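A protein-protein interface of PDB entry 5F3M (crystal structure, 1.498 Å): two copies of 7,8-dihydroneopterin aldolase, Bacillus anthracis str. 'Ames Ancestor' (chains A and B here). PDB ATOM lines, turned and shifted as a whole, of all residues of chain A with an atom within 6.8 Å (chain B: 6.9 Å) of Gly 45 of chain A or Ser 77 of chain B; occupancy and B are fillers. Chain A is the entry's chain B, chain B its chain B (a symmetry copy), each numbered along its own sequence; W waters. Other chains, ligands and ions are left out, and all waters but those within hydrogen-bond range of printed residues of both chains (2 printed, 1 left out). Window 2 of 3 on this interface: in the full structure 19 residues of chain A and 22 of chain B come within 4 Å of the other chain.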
ATOM      1  N   LEU A  41     -10.688  17.800 -11.091  1.00  0.00           N
ATOM      2  CA  LEU A  41     -11.428  18.566 -12.089  1.00  0.00           C
ATOM      3  C   LEU A  41     -10.569  19.026 -13.259  1.00  0.00           C
ATOM      4  O   LEU A  41     -11.092  19.665 -14.176  1.00  0.00           O
ATOM      5  CB  LEU A  41     -12.122  19.772 -11.443  1.00  0.00           C
ATOM      6  CG  LEU A  41     -13.189  19.435 -10.400  1.00  0.00           C
ATOM      7  CD1 LEU A  41     -13.754  20.702  -9.766  1.00  0.00           C
ATOM      8  CD2 LEU A  41     -14.301  18.630 -11.039  1.00  0.00           C
ATOM      9  N   LYS A  42      -9.272  18.707 -13.262  1.00  0.00           N
ATOM     10  CA  LYS A  42      -8.396  19.219 -14.315  1.00  0.00           C
ATOM     11  C   LYS A  42      -8.766  18.666 -15.691  1.00  0.00           C
ATOM     12  O   LYS A  42      -8.768  19.407 -16.681  1.00  0.00           O
ATOM     13  CB  LYS A  42      -6.928  18.945 -13.978  1.00  0.00           C
ATOM     14  CG  LYS A  42      -5.968  19.525 -14.996  1.00  0.00           C
ATOM     15  CD  LYS A  42      -4.519  19.291 -14.605  1.00  0.00           C
ATOM     16  CE  LYS A  42      -3.978  20.430 -13.765  1.00  0.00           C
ATOM     17  NZ  LYS A  42      -2.525  20.278 -13.477  1.00  0.00           N
ATOM     18  N   ARG A  43      -9.075  17.370 -15.780  1.00  0.00           N
ATOM     19  CA  ARG A  43      -9.451  16.812 -17.076  1.00  0.00           C
ATOM     20  C   ARG A  43     -10.713  17.474 -17.612  1.00  0.00           C
ATOM     21  O   ARG A  43     -10.824  17.730 -18.819  1.00  0.00           O
ATOM     22  CB  ARG A  43      -9.618  15.294 -16.980  1.00  0.00           C
ATOM     23  CG  ARG A  43      -8.323  14.557 -16.672  1.00  0.00           C
ATOM     24  CD  ARG A  43      -8.581  13.093 -16.339  1.00  0.00           C
ATOM     25  NE  ARG A  43      -8.669  12.247 -17.526  1.00  0.00           N
ATOM     26  CZ  ARG A  43      -8.998  10.958 -17.498  1.00  0.00           C
ATOM     27  NH1 ARG A  43      -9.046  10.255 -18.620  1.00  0.00           N
ATOM     28  NH2 ARG A  43      -9.288  10.372 -16.343  1.00  0.00           N
ATOM     29  N   ALA A  44     -11.671  17.769 -16.730  1.00  0.00           N
ATOM     30  CA  ALA A  44     -12.868  18.490 -17.153  1.00  0.00           C
ATOM     31  C   ALA A  44     -12.544  19.928 -17.555  1.00  0.00           C
ATOM     32  O   ALA A  44     -13.043  20.421 -18.574  1.00  0.00           O
ATOM     33  CB  ALA A  44     -13.897  18.491 -16.020  1.00  0.00           C
ATOM     34  N   GLY A  45     -11.723  20.621 -16.760  1.00  0.00           N
ATOM     35  CA  GLY A  45     -11.391  22.003 -17.073  1.00  0.00           C
ATOM     36  C   GLY A  45     -10.568  22.164 -18.339  1.00  0.00           C
ATOM     37  O   GLY A  45     -10.604  23.224 -18.976  1.00  0.00           O
ATOM     38  N   GLU A  46      -9.812  21.130 -18.721  1.00  0.00           N
ATOM     39  CA  GLU A  46      -9.042  21.175 -19.961  1.00  0.00           C
ATOM     40  C   GLU A  46      -9.873  20.804 -21.184  1.00  0.00           C
ATOM     41  O   GLU A  46      -9.652  21.361 -22.265  1.00  0.00           O
ATOM     42  CB  GLU A  46      -7.822  20.257 -19.851  1.00  0.00           C
ATOM     43  CG  GLU A  46      -6.800  20.795 -18.880  1.00  0.00           C
ATOM     44  CD  GLU A  46      -5.596  19.900 -18.701  1.00  0.00           C
ATOM     45  OE1 GLU A  46      -5.606  18.743 -19.183  1.00  0.00           O
ATOM     46  OE2 GLU A  46      -4.627  20.367 -18.069  1.00  0.00           O
ATOM     47  N   SER A  47     -10.820  19.877 -21.036  1.00  0.00           N
ATOM     48  CA  SER A  47     -11.586  19.351 -22.158  1.00  0.00           C
ATOM     49  C   SER A  47     -12.928  20.032 -22.359  1.00  0.00           C
ATOM     50  O   SER A  47     -13.490  19.933 -23.458  1.00  0.00           O
ATOM     51  CB  SER A  47     -11.867  17.860 -21.945  1.00  0.00           C
ATOM     52  OG  SER A  47     -12.688  17.685 -20.797  1.00  0.00           O
ATOM     53  N   ASP A  48     -13.462  20.698 -21.333  1.00  0.00           N
ATOM     54  CA  ASP A  48     -14.831  21.216 -21.339  1.00  0.00           C
ATOM     55  C   ASP A  48     -15.876  20.102 -21.476  1.00  0.00           C
ATOM     56  O   ASP A  48     -17.001  20.357 -21.917  1.00  0.00           O
ATOM     57  CB  ASP A  48     -15.022  22.310 -22.409  1.00  0.00           C
ATOM     58  CG  ASP A  48     -16.137  23.290 -22.076  1.00  0.00           C
ATOM     59  OD1 ASP A  48     -16.333  23.606 -20.887  1.00  0.00           O
ATOM     60  OD2 ASP A  48     -16.809  23.768 -23.020  1.00  0.00           O
ATOM     61  N   ASP A  49     -15.526  18.875 -21.091  1.00  0.00           N
ATOM     62  CA  ASP A  49     -16.391  17.710 -21.245  1.00  0.00           C
ATOM     63  C   ASP A  49     -16.930  17.310 -19.877  1.00  0.00           C
ATOM     64  O   ASP A  49     -16.160  16.919 -18.993  1.00  0.00           O
ATOM     65  CB  ASP A  49     -15.607  16.549 -21.858  1.00  0.00           C
ATOM     66  CG  ASP A  49     -16.498  15.398 -22.295  1.00  0.00           C
ATOM     67  OD1 ASP A  49     -17.644  15.272 -21.804  1.00  0.00           O
ATOM     68  OD2 ASP A  49     -16.038  14.597 -23.132  1.00  0.00           O
ATOM     69  N   HIS A  52     -16.000  14.192 -17.630  1.00  0.00           N
ATOM     70  CA  HIS A  52     -14.849  14.187 -16.734  1.00  0.00           C
ATOM     71  C   HIS A  52     -15.150  14.797 -15.371  1.00  0.00           C
ATOM     72  O   HIS A  52     -14.233  14.946 -14.555  1.00  0.00           O
ATOM     73  CB  HIS A  52     -13.655  14.908 -17.372  1.00  0.00           C
ATOM     74  CG  HIS A  52     -12.978  14.111 -18.442  1.00  0.00           C
ATOM     75  ND1 HIS A  52     -12.280  12.952 -18.177  1.00  0.00           N
ATOM     76  CD2 HIS A  52     -12.898  14.303 -19.780  1.00  0.00           C
ATOM     77  CE1 HIS A  52     -11.795  12.465 -19.308  1.00  0.00           C
ATOM     78  NE2 HIS A  52     -12.155  13.266 -20.297  1.00  0.00           N
ATOM     79  N   HIS B  18     -22.004  30.892 -20.169  1.00  0.00           N
ATOM     80  CA  HIS B  18     -21.526  29.525 -20.055  1.00  0.00           C
ATOM     81  C   HIS B  18     -22.660  28.589 -19.672  1.00  0.00           C
ATOM     82  O   HIS B  18     -23.635  28.986 -19.026  1.00  0.00           O
ATOM     83  CB  HIS B  18     -20.442  29.456 -18.989  1.00  0.00           C
ATOM     84  CG  HIS B  18     -19.436  30.558 -19.096  1.00  0.00           C
ATOM     85  ND1 HIS B  18     -18.324  30.474 -19.908  1.00  0.00           N
ATOM     86  CD2 HIS B  18     -19.386  31.781 -18.513  1.00  0.00           C
ATOM     87  CE1 HIS B  18     -17.631  31.595 -19.817  1.00  0.00           C
ATOM     88  NE2 HIS B  18     -18.253  32.403 -18.974  1.00  0.00           N
ATOM     89  N   VAL B  66     -11.914  36.011 -18.998  1.00  0.00           N
ATOM     90  CA  VAL B  66     -12.321  34.612 -19.104  1.00  0.00           C
ATOM     91  C   VAL B  66     -13.837  34.473 -18.999  1.00  0.00           C
ATOM     92  O   VAL B  66     -14.454  33.722 -19.765  1.00  0.00           O
ATOM     93  CB  VAL B  66     -11.588  33.737 -18.072  1.00  0.00           C
ATOM     94  CG1 VAL B  66     -12.070  32.289 -18.168  1.00  0.00           C
ATOM     95  CG2 VAL B  66     -10.076  33.809 -18.281  1.00  0.00           C
ATOM     96  N   ARG B  70     -15.409  34.881 -23.228  1.00  0.00           N
ATOM     97  CA  ARG B  70     -15.382  33.509 -23.708  1.00  0.00           C
ATOM     98  C   ARG B  70     -16.654  32.818 -23.243  1.00  0.00           C
ATOM     99  O   ARG B  70     -17.321  33.274 -22.314  1.00  0.00           O
ATOM    100  CB  ARG B  70     -14.178  32.747 -23.138  1.00  0.00           C
ATOM    101  CG  ARG B  70     -12.854  33.484 -23.257  1.00  0.00           C
ATOM    102  CD  ARG B  70     -11.737  32.667 -22.656  1.00  0.00           C
ATOM    103  NE  ARG B  70     -10.525  33.451 -22.438  1.00  0.00           N
ATOM    104  CZ  ARG B  70      -9.430  32.975 -21.854  1.00  0.00           C
ATOM    105  NH1 ARG B  70      -9.402  31.717 -21.435  1.00  0.00           N
ATOM    106  NH2 ARG B  70      -8.365  33.753 -21.690  1.00  0.00           N
ATOM    107  N   TYR B  72     -17.875  28.804 -22.352  1.00  0.00           N
ATOM    108  CA  TYR B  72     -17.595  27.388 -22.178  1.00  0.00           C
ATOM    109  C   TYR B  72     -18.857  26.666 -21.734  1.00  0.00           C
ATOM    110  O   TYR B  72     -19.822  27.280 -21.270  1.00  0.00           O
ATOM    111  CB  TYR B  72     -16.555  27.172 -21.066  1.00  0.00           C
ATOM    112  CG  TYR B  72     -15.221  27.823 -21.317  1.00  0.00           C
ATOM    113  CD1 TYR B  72     -14.344  27.307 -22.258  1.00  0.00           C
ATOM    114  CD2 TYR B  72     -14.826  28.943 -20.599  1.00  0.00           C
ATOM    115  CE1 TYR B  72     -13.114  27.895 -22.485  1.00  0.00           C
ATOM    116  CE2 TYR B  72     -13.601  29.535 -20.819  1.00  0.00           C
ATOM    117  CZ  TYR B  72     -12.751  29.012 -21.764  1.00  0.00           C
ATOM    118  OH  TYR B  72     -11.526  29.607 -21.979  1.00  0.00           O
ATOM    119  N   LYS B  73     -18.852  25.342 -21.872  1.00  0.00           N
ATOM    120  CA  LYS B  73     -19.949  24.569 -21.299  1.00  0.00           C
ATOM    121  C   LYS B  73     -19.862  24.536 -19.779  1.00  0.00           C
ATOM    122  O   LYS B  73     -20.873  24.734 -19.091  1.00  0.00           O
ATOM    123  CB  LYS B  73     -19.968  23.146 -21.860  1.00  0.00           C
ATOM    124  CG  LYS B  73     -20.448  23.052 -23.300  1.00  0.00           C
ATOM    125  CD  LYS B  73     -20.625  21.603 -23.732  1.00  0.00           C
ATOM    126  CE  LYS B  73     -21.095  21.524 -25.176  1.00  0.00           C
ATOM    127  NZ  LYS B  73     -20.137  22.194 -26.095  1.00  0.00           N
ATOM    128  N   LEU B  74     -18.666  24.309 -19.235  1.00  0.00           N
ATOM    129  CA  LEU B  74     -18.492  23.979 -17.824  1.00  0.00           C
ATOM    130  C   LEU B  74     -17.882  25.117 -17.019  1.00  0.00           C
ATOM    131  O   LEU B  74     -16.954  25.796 -17.480  1.00  0.00           O
ATOM    132  CB  LEU B  74     -17.557  22.767 -17.659  1.00  0.00           C
ATOM    133  CG  LEU B  74     -17.922  21.460 -18.357  1.00  0.00           C
ATOM    134  CD1 LEU B  74     -16.918  20.364 -17.992  1.00  0.00           C
ATOM    135  CD2 LEU B  74     -19.356  21.041 -18.019  1.00  0.00           C
ATOM    136  N   VAL B  75     -18.349  25.266 -15.773  1.00  0.00           N
ATOM    137  CA  VAL B  75     -17.677  26.188 -14.858  1.00  0.00           C
ATOM    138  C   VAL B  75     -16.249  25.734 -14.576  1.00  0.00           C
ATOM    139  O   VAL B  75     -15.370  26.563 -14.309  1.00  0.00           O
ATOM    140  CB  VAL B  75     -18.488  26.427 -13.567  1.00  0.00           C
ATOM    141  CG1 VAL B  75     -19.737  27.236 -13.870  1.00  0.00           C
ATOM    142  CG2 VAL B  75     -18.869  25.124 -12.912  1.00  0.00           C
ATOM    143  N   GLU B  76     -15.987  24.420 -14.651  1.00  0.00           N
ATOM    144  CA  GLU B  76     -14.625  23.913 -14.513  1.00  0.00           C
ATOM    145  C   GLU B  76     -13.681  24.574 -15.514  1.00  0.00           C
ATOM    146  O   GLU B  76     -12.523  24.868 -15.188  1.00  0.00           O
ATOM    147  CB  GLU B  76     -14.612  22.395 -14.728  1.00  0.00           C
ATOM    148  CG  GLU B  76     -15.169  21.558 -13.568  1.00  0.00           C
ATOM    149  CD  GLU B  76     -16.683  21.353 -13.585  1.00  0.00           C
ATOM    150  OE1 GLU B  76     -17.421  22.123 -14.245  1.00  0.00           O
ATOM    151  OE2 GLU B  76     -17.143  20.401 -12.911  1.00  0.00           O
ATOM    152  N   SER B  77     -14.160  24.813 -16.741  1.00  0.00           N
ATOM    153  CA  SER B  77     -13.322  25.437 -17.760  1.00  0.00           C
ATOM    154  C   SER B  77     -13.021  26.889 -17.422  1.00  0.00           C
ATOM    155  O   SER B  77     -11.923  27.381 -17.710  1.00  0.00           O
ATOM    156  CB  SER B  77     -13.986  25.337 -19.133  1.00  0.00           C
ATOM    157  OG  SER B  77     -14.080  23.988 -19.534  1.00  0.00           O
ATOM    158  N   ILE B  78     -13.987  27.597 -16.828  1.00  0.00           N
ATOM    159  CA  ILE B  78     -13.726  28.964 -16.381  1.00  0.00           C
ATOM    160  C   ILE B  78     -12.603  28.964 -15.354  1.00  0.00           C
ATOM    161  O   ILE B  78     -11.624  29.711 -15.471  1.00  0.00           O
ATOM    162  CB  ILE B  78     -15.003  29.606 -15.804  1.00  0.00           C
ATOM    163  CG1 ILE B  78     -16.148  29.613 -16.827  1.00  0.00           C
ATOM    164  CG2 ILE B  78     -14.724  31.027 -15.306  1.00  0.00           C
ATOM    165  CD1 ILE B  78     -17.490  30.005 -16.209  1.00  0.00           C
ATOM    166  N   ALA B  79     -12.736  28.121 -14.325  1.00  0.00           N
ATOM    167  CA  ALA B  79     -11.741  28.074 -13.255  1.00  0.00           C
ATOM    168  C   ALA B  79     -10.366  27.708 -13.799  1.00  0.00           C
ATOM    169  O   ALA B  79      -9.361  28.348 -13.468  1.00  0.00           O
ATOM    170  CB  ALA B  79     -12.181  27.074 -12.183  1.00  0.00           C
ATOM    171  N   GLU B  80     -10.311  26.689 -14.660  1.00  0.00           N
ATOM    172  CA  GLU B  80      -9.025  26.206 -15.162  1.00  0.00           C
ATOM    173  C   GLU B  80      -8.331  27.268 -16.001  1.00  0.00           C
ATOM    174  O   GLU B  80      -7.111  27.449 -15.902  1.00  0.00           O
ATOM    175  CB  GLU B  80      -9.232  24.935 -15.980  1.00  0.00           C
ATOM    176  CG  GLU B  80      -7.953  24.146 -16.203  1.00  0.00           C
ATOM    177  CD  GLU B  80      -7.512  23.391 -14.960  1.00  0.00           C
ATOM    178  OE1 GLU B  80      -8.389  22.896 -14.220  1.00  0.00           O
ATOM    179  OE2 GLU B  80      -6.289  23.290 -14.717  1.00  0.00           O
ATOM    180  N   ASN B  81      -9.092  27.994 -16.822  1.00  0.00           N
ATOM    181  CA  ASN B  81      -8.474  29.002 -17.674  1.00  0.00           C
ATOM    182  C   ASN B  81      -7.993  30.205 -16.871  1.00  0.00           C
ATOM    183  O   ASN B  81      -6.932  30.766 -17.174  1.00  0.00           O
ATOM    184  CB  ASN B  81      -9.415  29.393 -18.806  1.00  0.00           C
ATOM    185  CG  ASN B  81      -9.319  28.424 -19.972  1.00  0.00           C
ATOM    186  OD1 ASN B  81      -8.425  28.541 -20.814  1.00  0.00           O
ATOM    187  ND2 ASN B  81     -10.217  27.437 -20.010  1.00  0.00           N
ATOM    188  N   ILE B  82      -8.750  30.618 -15.848  1.00  0.00           N
ATOM    189  CA  ILE B  82      -8.278  31.694 -14.976  1.00  0.00           C
ATOM    190  C   ILE B  82      -6.965  31.300 -14.307  1.00  0.00           C
ATOM    191  O   ILE B  82      -5.992  32.066 -14.317  1.00  0.00           O
ATOM    192  CB  ILE B  82      -9.353  32.091 -13.948  1.00  0.00           C
ATOM    193  CG1 ILE B  82     -10.546  32.754 -14.649  1.00  0.00           C
ATOM    194  CG2 ILE B  82      -8.752  33.041 -12.906  1.00  0.00           C
ATOM    195  CD1 ILE B  82     -11.718  33.051 -13.708  1.00  0.00           C
ATOM    196  N   VAL B 100     -15.313  29.373  -8.841  1.00  0.00           N
ATOM    197  CA  VAL B 100     -16.289  29.897  -9.795  1.00  0.00           C
ATOM    198  C   VAL B 100     -17.672  29.463  -9.328  1.00  0.00           C
ATOM    199  O   VAL B 100     -17.924  28.264  -9.133  1.00  0.00           O
ATOM    200  CB  VAL B 100     -16.003  29.436 -11.232  1.00  0.00           C
ATOM    201  CG1 VAL B 100     -17.068  29.958 -12.182  1.00  0.00           C
ATOM    202  CG2 VAL B 100     -14.610  29.891 -11.670  1.00  0.00           C
ATOM    203  N   VAL B 116     -17.471  25.451  -8.279  1.00  0.00           N
ATOM    204  CA  VAL B 116     -16.274  24.625  -8.361  1.00  0.00           C
ATOM    205  C   VAL B 116     -15.106  25.421  -7.800  1.00  0.00           C
ATOM    206  O   VAL B 116     -15.075  26.654  -7.875  1.00  0.00           O
ATOM    207  CB  VAL B 116     -15.947  24.136  -9.791  1.00  0.00           C
ATOM    208  CG1 VAL B 116     -17.050  23.232 -10.332  1.00  0.00           C
ATOM    209  CG2 VAL B 116     -15.653  25.308 -10.716  1.00  0.00           C
ATOM    210  N   ARG B 120      -4.081  25.528  -8.053  1.00  0.00           N
ATOM    211  CA  ARG B 120      -3.109  25.199  -9.091  1.00  0.00           C
ATOM    212  C   ARG B 120      -1.758  25.820  -8.776  1.00  0.00           C
ATOM    213  O   ARG B 120      -1.680  26.948  -8.275  1.00  0.00           O
ATOM    214  CB  ARG B 120      -3.577  25.685 -10.469  1.00  0.00           C
ATOM    215  CG  ARG B 120      -4.836  24.997 -10.974  1.00  0.00           C
ATOM    216  CD  ARG B 120      -4.560  23.554 -11.415  1.00  0.00           C
ATOM    217  NE  ARG B 120      -5.775  22.904 -11.902  1.00  0.00           N
ATOM    218  CZ  ARG B 120      -6.586  22.163 -11.149  1.00  0.00           C
ATOM    219  NH1 ARG B 120      -6.305  21.946  -9.867  1.00  0.00           N
ATOM    220  NH2 ARG B 120      -7.676  21.628 -11.683  1.00  0.00           N
HETATM  221  O   HOH W   1      -4.601  22.712 -16.763  1.00  0.00           O
HETATM  222  O   HOH W   2     -11.823  23.997 -21.378  1.00  0.00           O
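The backbone NH (N) of Lys 73 of chain B lies within hydrogen-bond range of the side-chain carboxylate (OD2) of Asp 48 of chain A, at 2.8 Å.
The side-chain carboxylate of Asp 48 of chain A lies within hydrogen-bond range of the backbone NH of Leu 74 of chain B (2.9 Å).
The side-chain hydroxyl (OG) of Ser 77 of chain B is in hydrogen-bond range of the side-chain carboxylate (OD1) of Asp 48 of chain A.
The guanidinium group (NH1) of Arg 70 of chain B sits at hydrogen-bond distance from the side-chain hydroxyl (OH) of Tyr 72 of chain B, 3.0 Å away.
The backbone carbonyl oxygen (O) of Ser 77 of chain B sits at hydrogen-bond distance from the side-chain amide nitrogen (ND2) of Asn 81 of chain B, 2.9 Å away.
ND1 of His 18 of chain B lies within hydrogen-bond range of N of Tyr 72 of chain B (3.0 Å).
The side-chain carboxylate of Glu 80 of chain B is in salt-bridge range of the guanidinium group of Arg 120 of chain B, 2.9 Å away.
The side-chain hydroxyl (OH) of Tyr 72 of chain B sits close to the side-chain amide nitrogen (ND2) of Asn 81 of chain B.
OG of Ser 47 of chain A lies within hydrogen-bond range of N of Asp 49 of chain A (3.1 Å).
Among the printed residues, pairs that only touch across the chains: Asp 48 of chain A with Tyr 72 of chain B, Lys 42 of chain A with Arg 120 of chain B, Asp 49 of chain A with Leu 74 of chain B, Gly 45 of chain A with Ser 77 of chain B, Gly 45 of chain A with Glu 76 of chain B, Lys 42 of chain A with Glu 80 of chain B, Gly 45 of chain A with Glu 80 of chain B, Leu 41 of chain A with Glu 76 of chain B, Ala 44 of chain A with Ser 77 of chain B and Ala 44 of chain A with Leu 74 of chain B.
Gly 45 of chain A touches just these residues of chain B: Glu 76, Ser 77 and Glu 80.
Printed residues of chain B within 4 Å of Asp 49 of chain A: Leu 74.
Printed residues of chain A within 4 Å of Leu 74 of chain B: Ala 44, Asp 48 and Asp 49.
Of the printed residues of chain A, Glu 76 of chain B touches Leu 41 and Gly 45.
Ala 79 of chain B touches none of the printed residues of chain A.
Asn 81 of chain B touches none of the printed residues of chain A.
The nearest residue of chain B that does not touch Gly 45 of chain A is Asn 81 of chain B (4.4 Å).
The nearest printed residue of chain A that does not touch Lys 73 of chain B is Asp 49 of chain A (6.2 Å).
Printed residues of chain A that touch a printed residue of chain B: Leu 41, Lys 42, Ala 44, Gly 45, Asp 48 and Asp 49.
Along chain A the printed residues that touch a printed residue of chain B span positions 41 to 49.
Of the 17 printed residues of chain B, 7 touch a printed residue of chain A.
Printed residues of chain B that touch a printed residue of chain A: Tyr 72, Lys 73, Leu 74, Glu 76, Ser 77, Glu 80 and Arg 120.
Hydrophobic or aromatic side chains of chain B within 4 Å of the printed part of chain A: Tyr 72 and Leu 74.
Among the printed residues, 13 pairs touch across the chains.
Among the printed residues, no Asp or Glu carboxylate lies within 4 Å of a Lys or Arg side-chain nitrogen of the other chain.
No position is printed for both chains.
Of the 13 pairs that touch across the chains among the printed residues, none has its exchanged pair printed and touching as well.
Water W1 bridges the side-chain carboxylate (OE2) of Glu 46 of chain A (2.7 Å) and the side-chain carboxylate (OE2) of Glu 80 of chain B (2.7 Å).
Water W2 bridges the backbone carbonyl oxygen (O) of Gly 45 of chain A (2.8 Å) and the side-chain hydroxyl (OG) of Ser 77 of chain B (2.9 Å).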
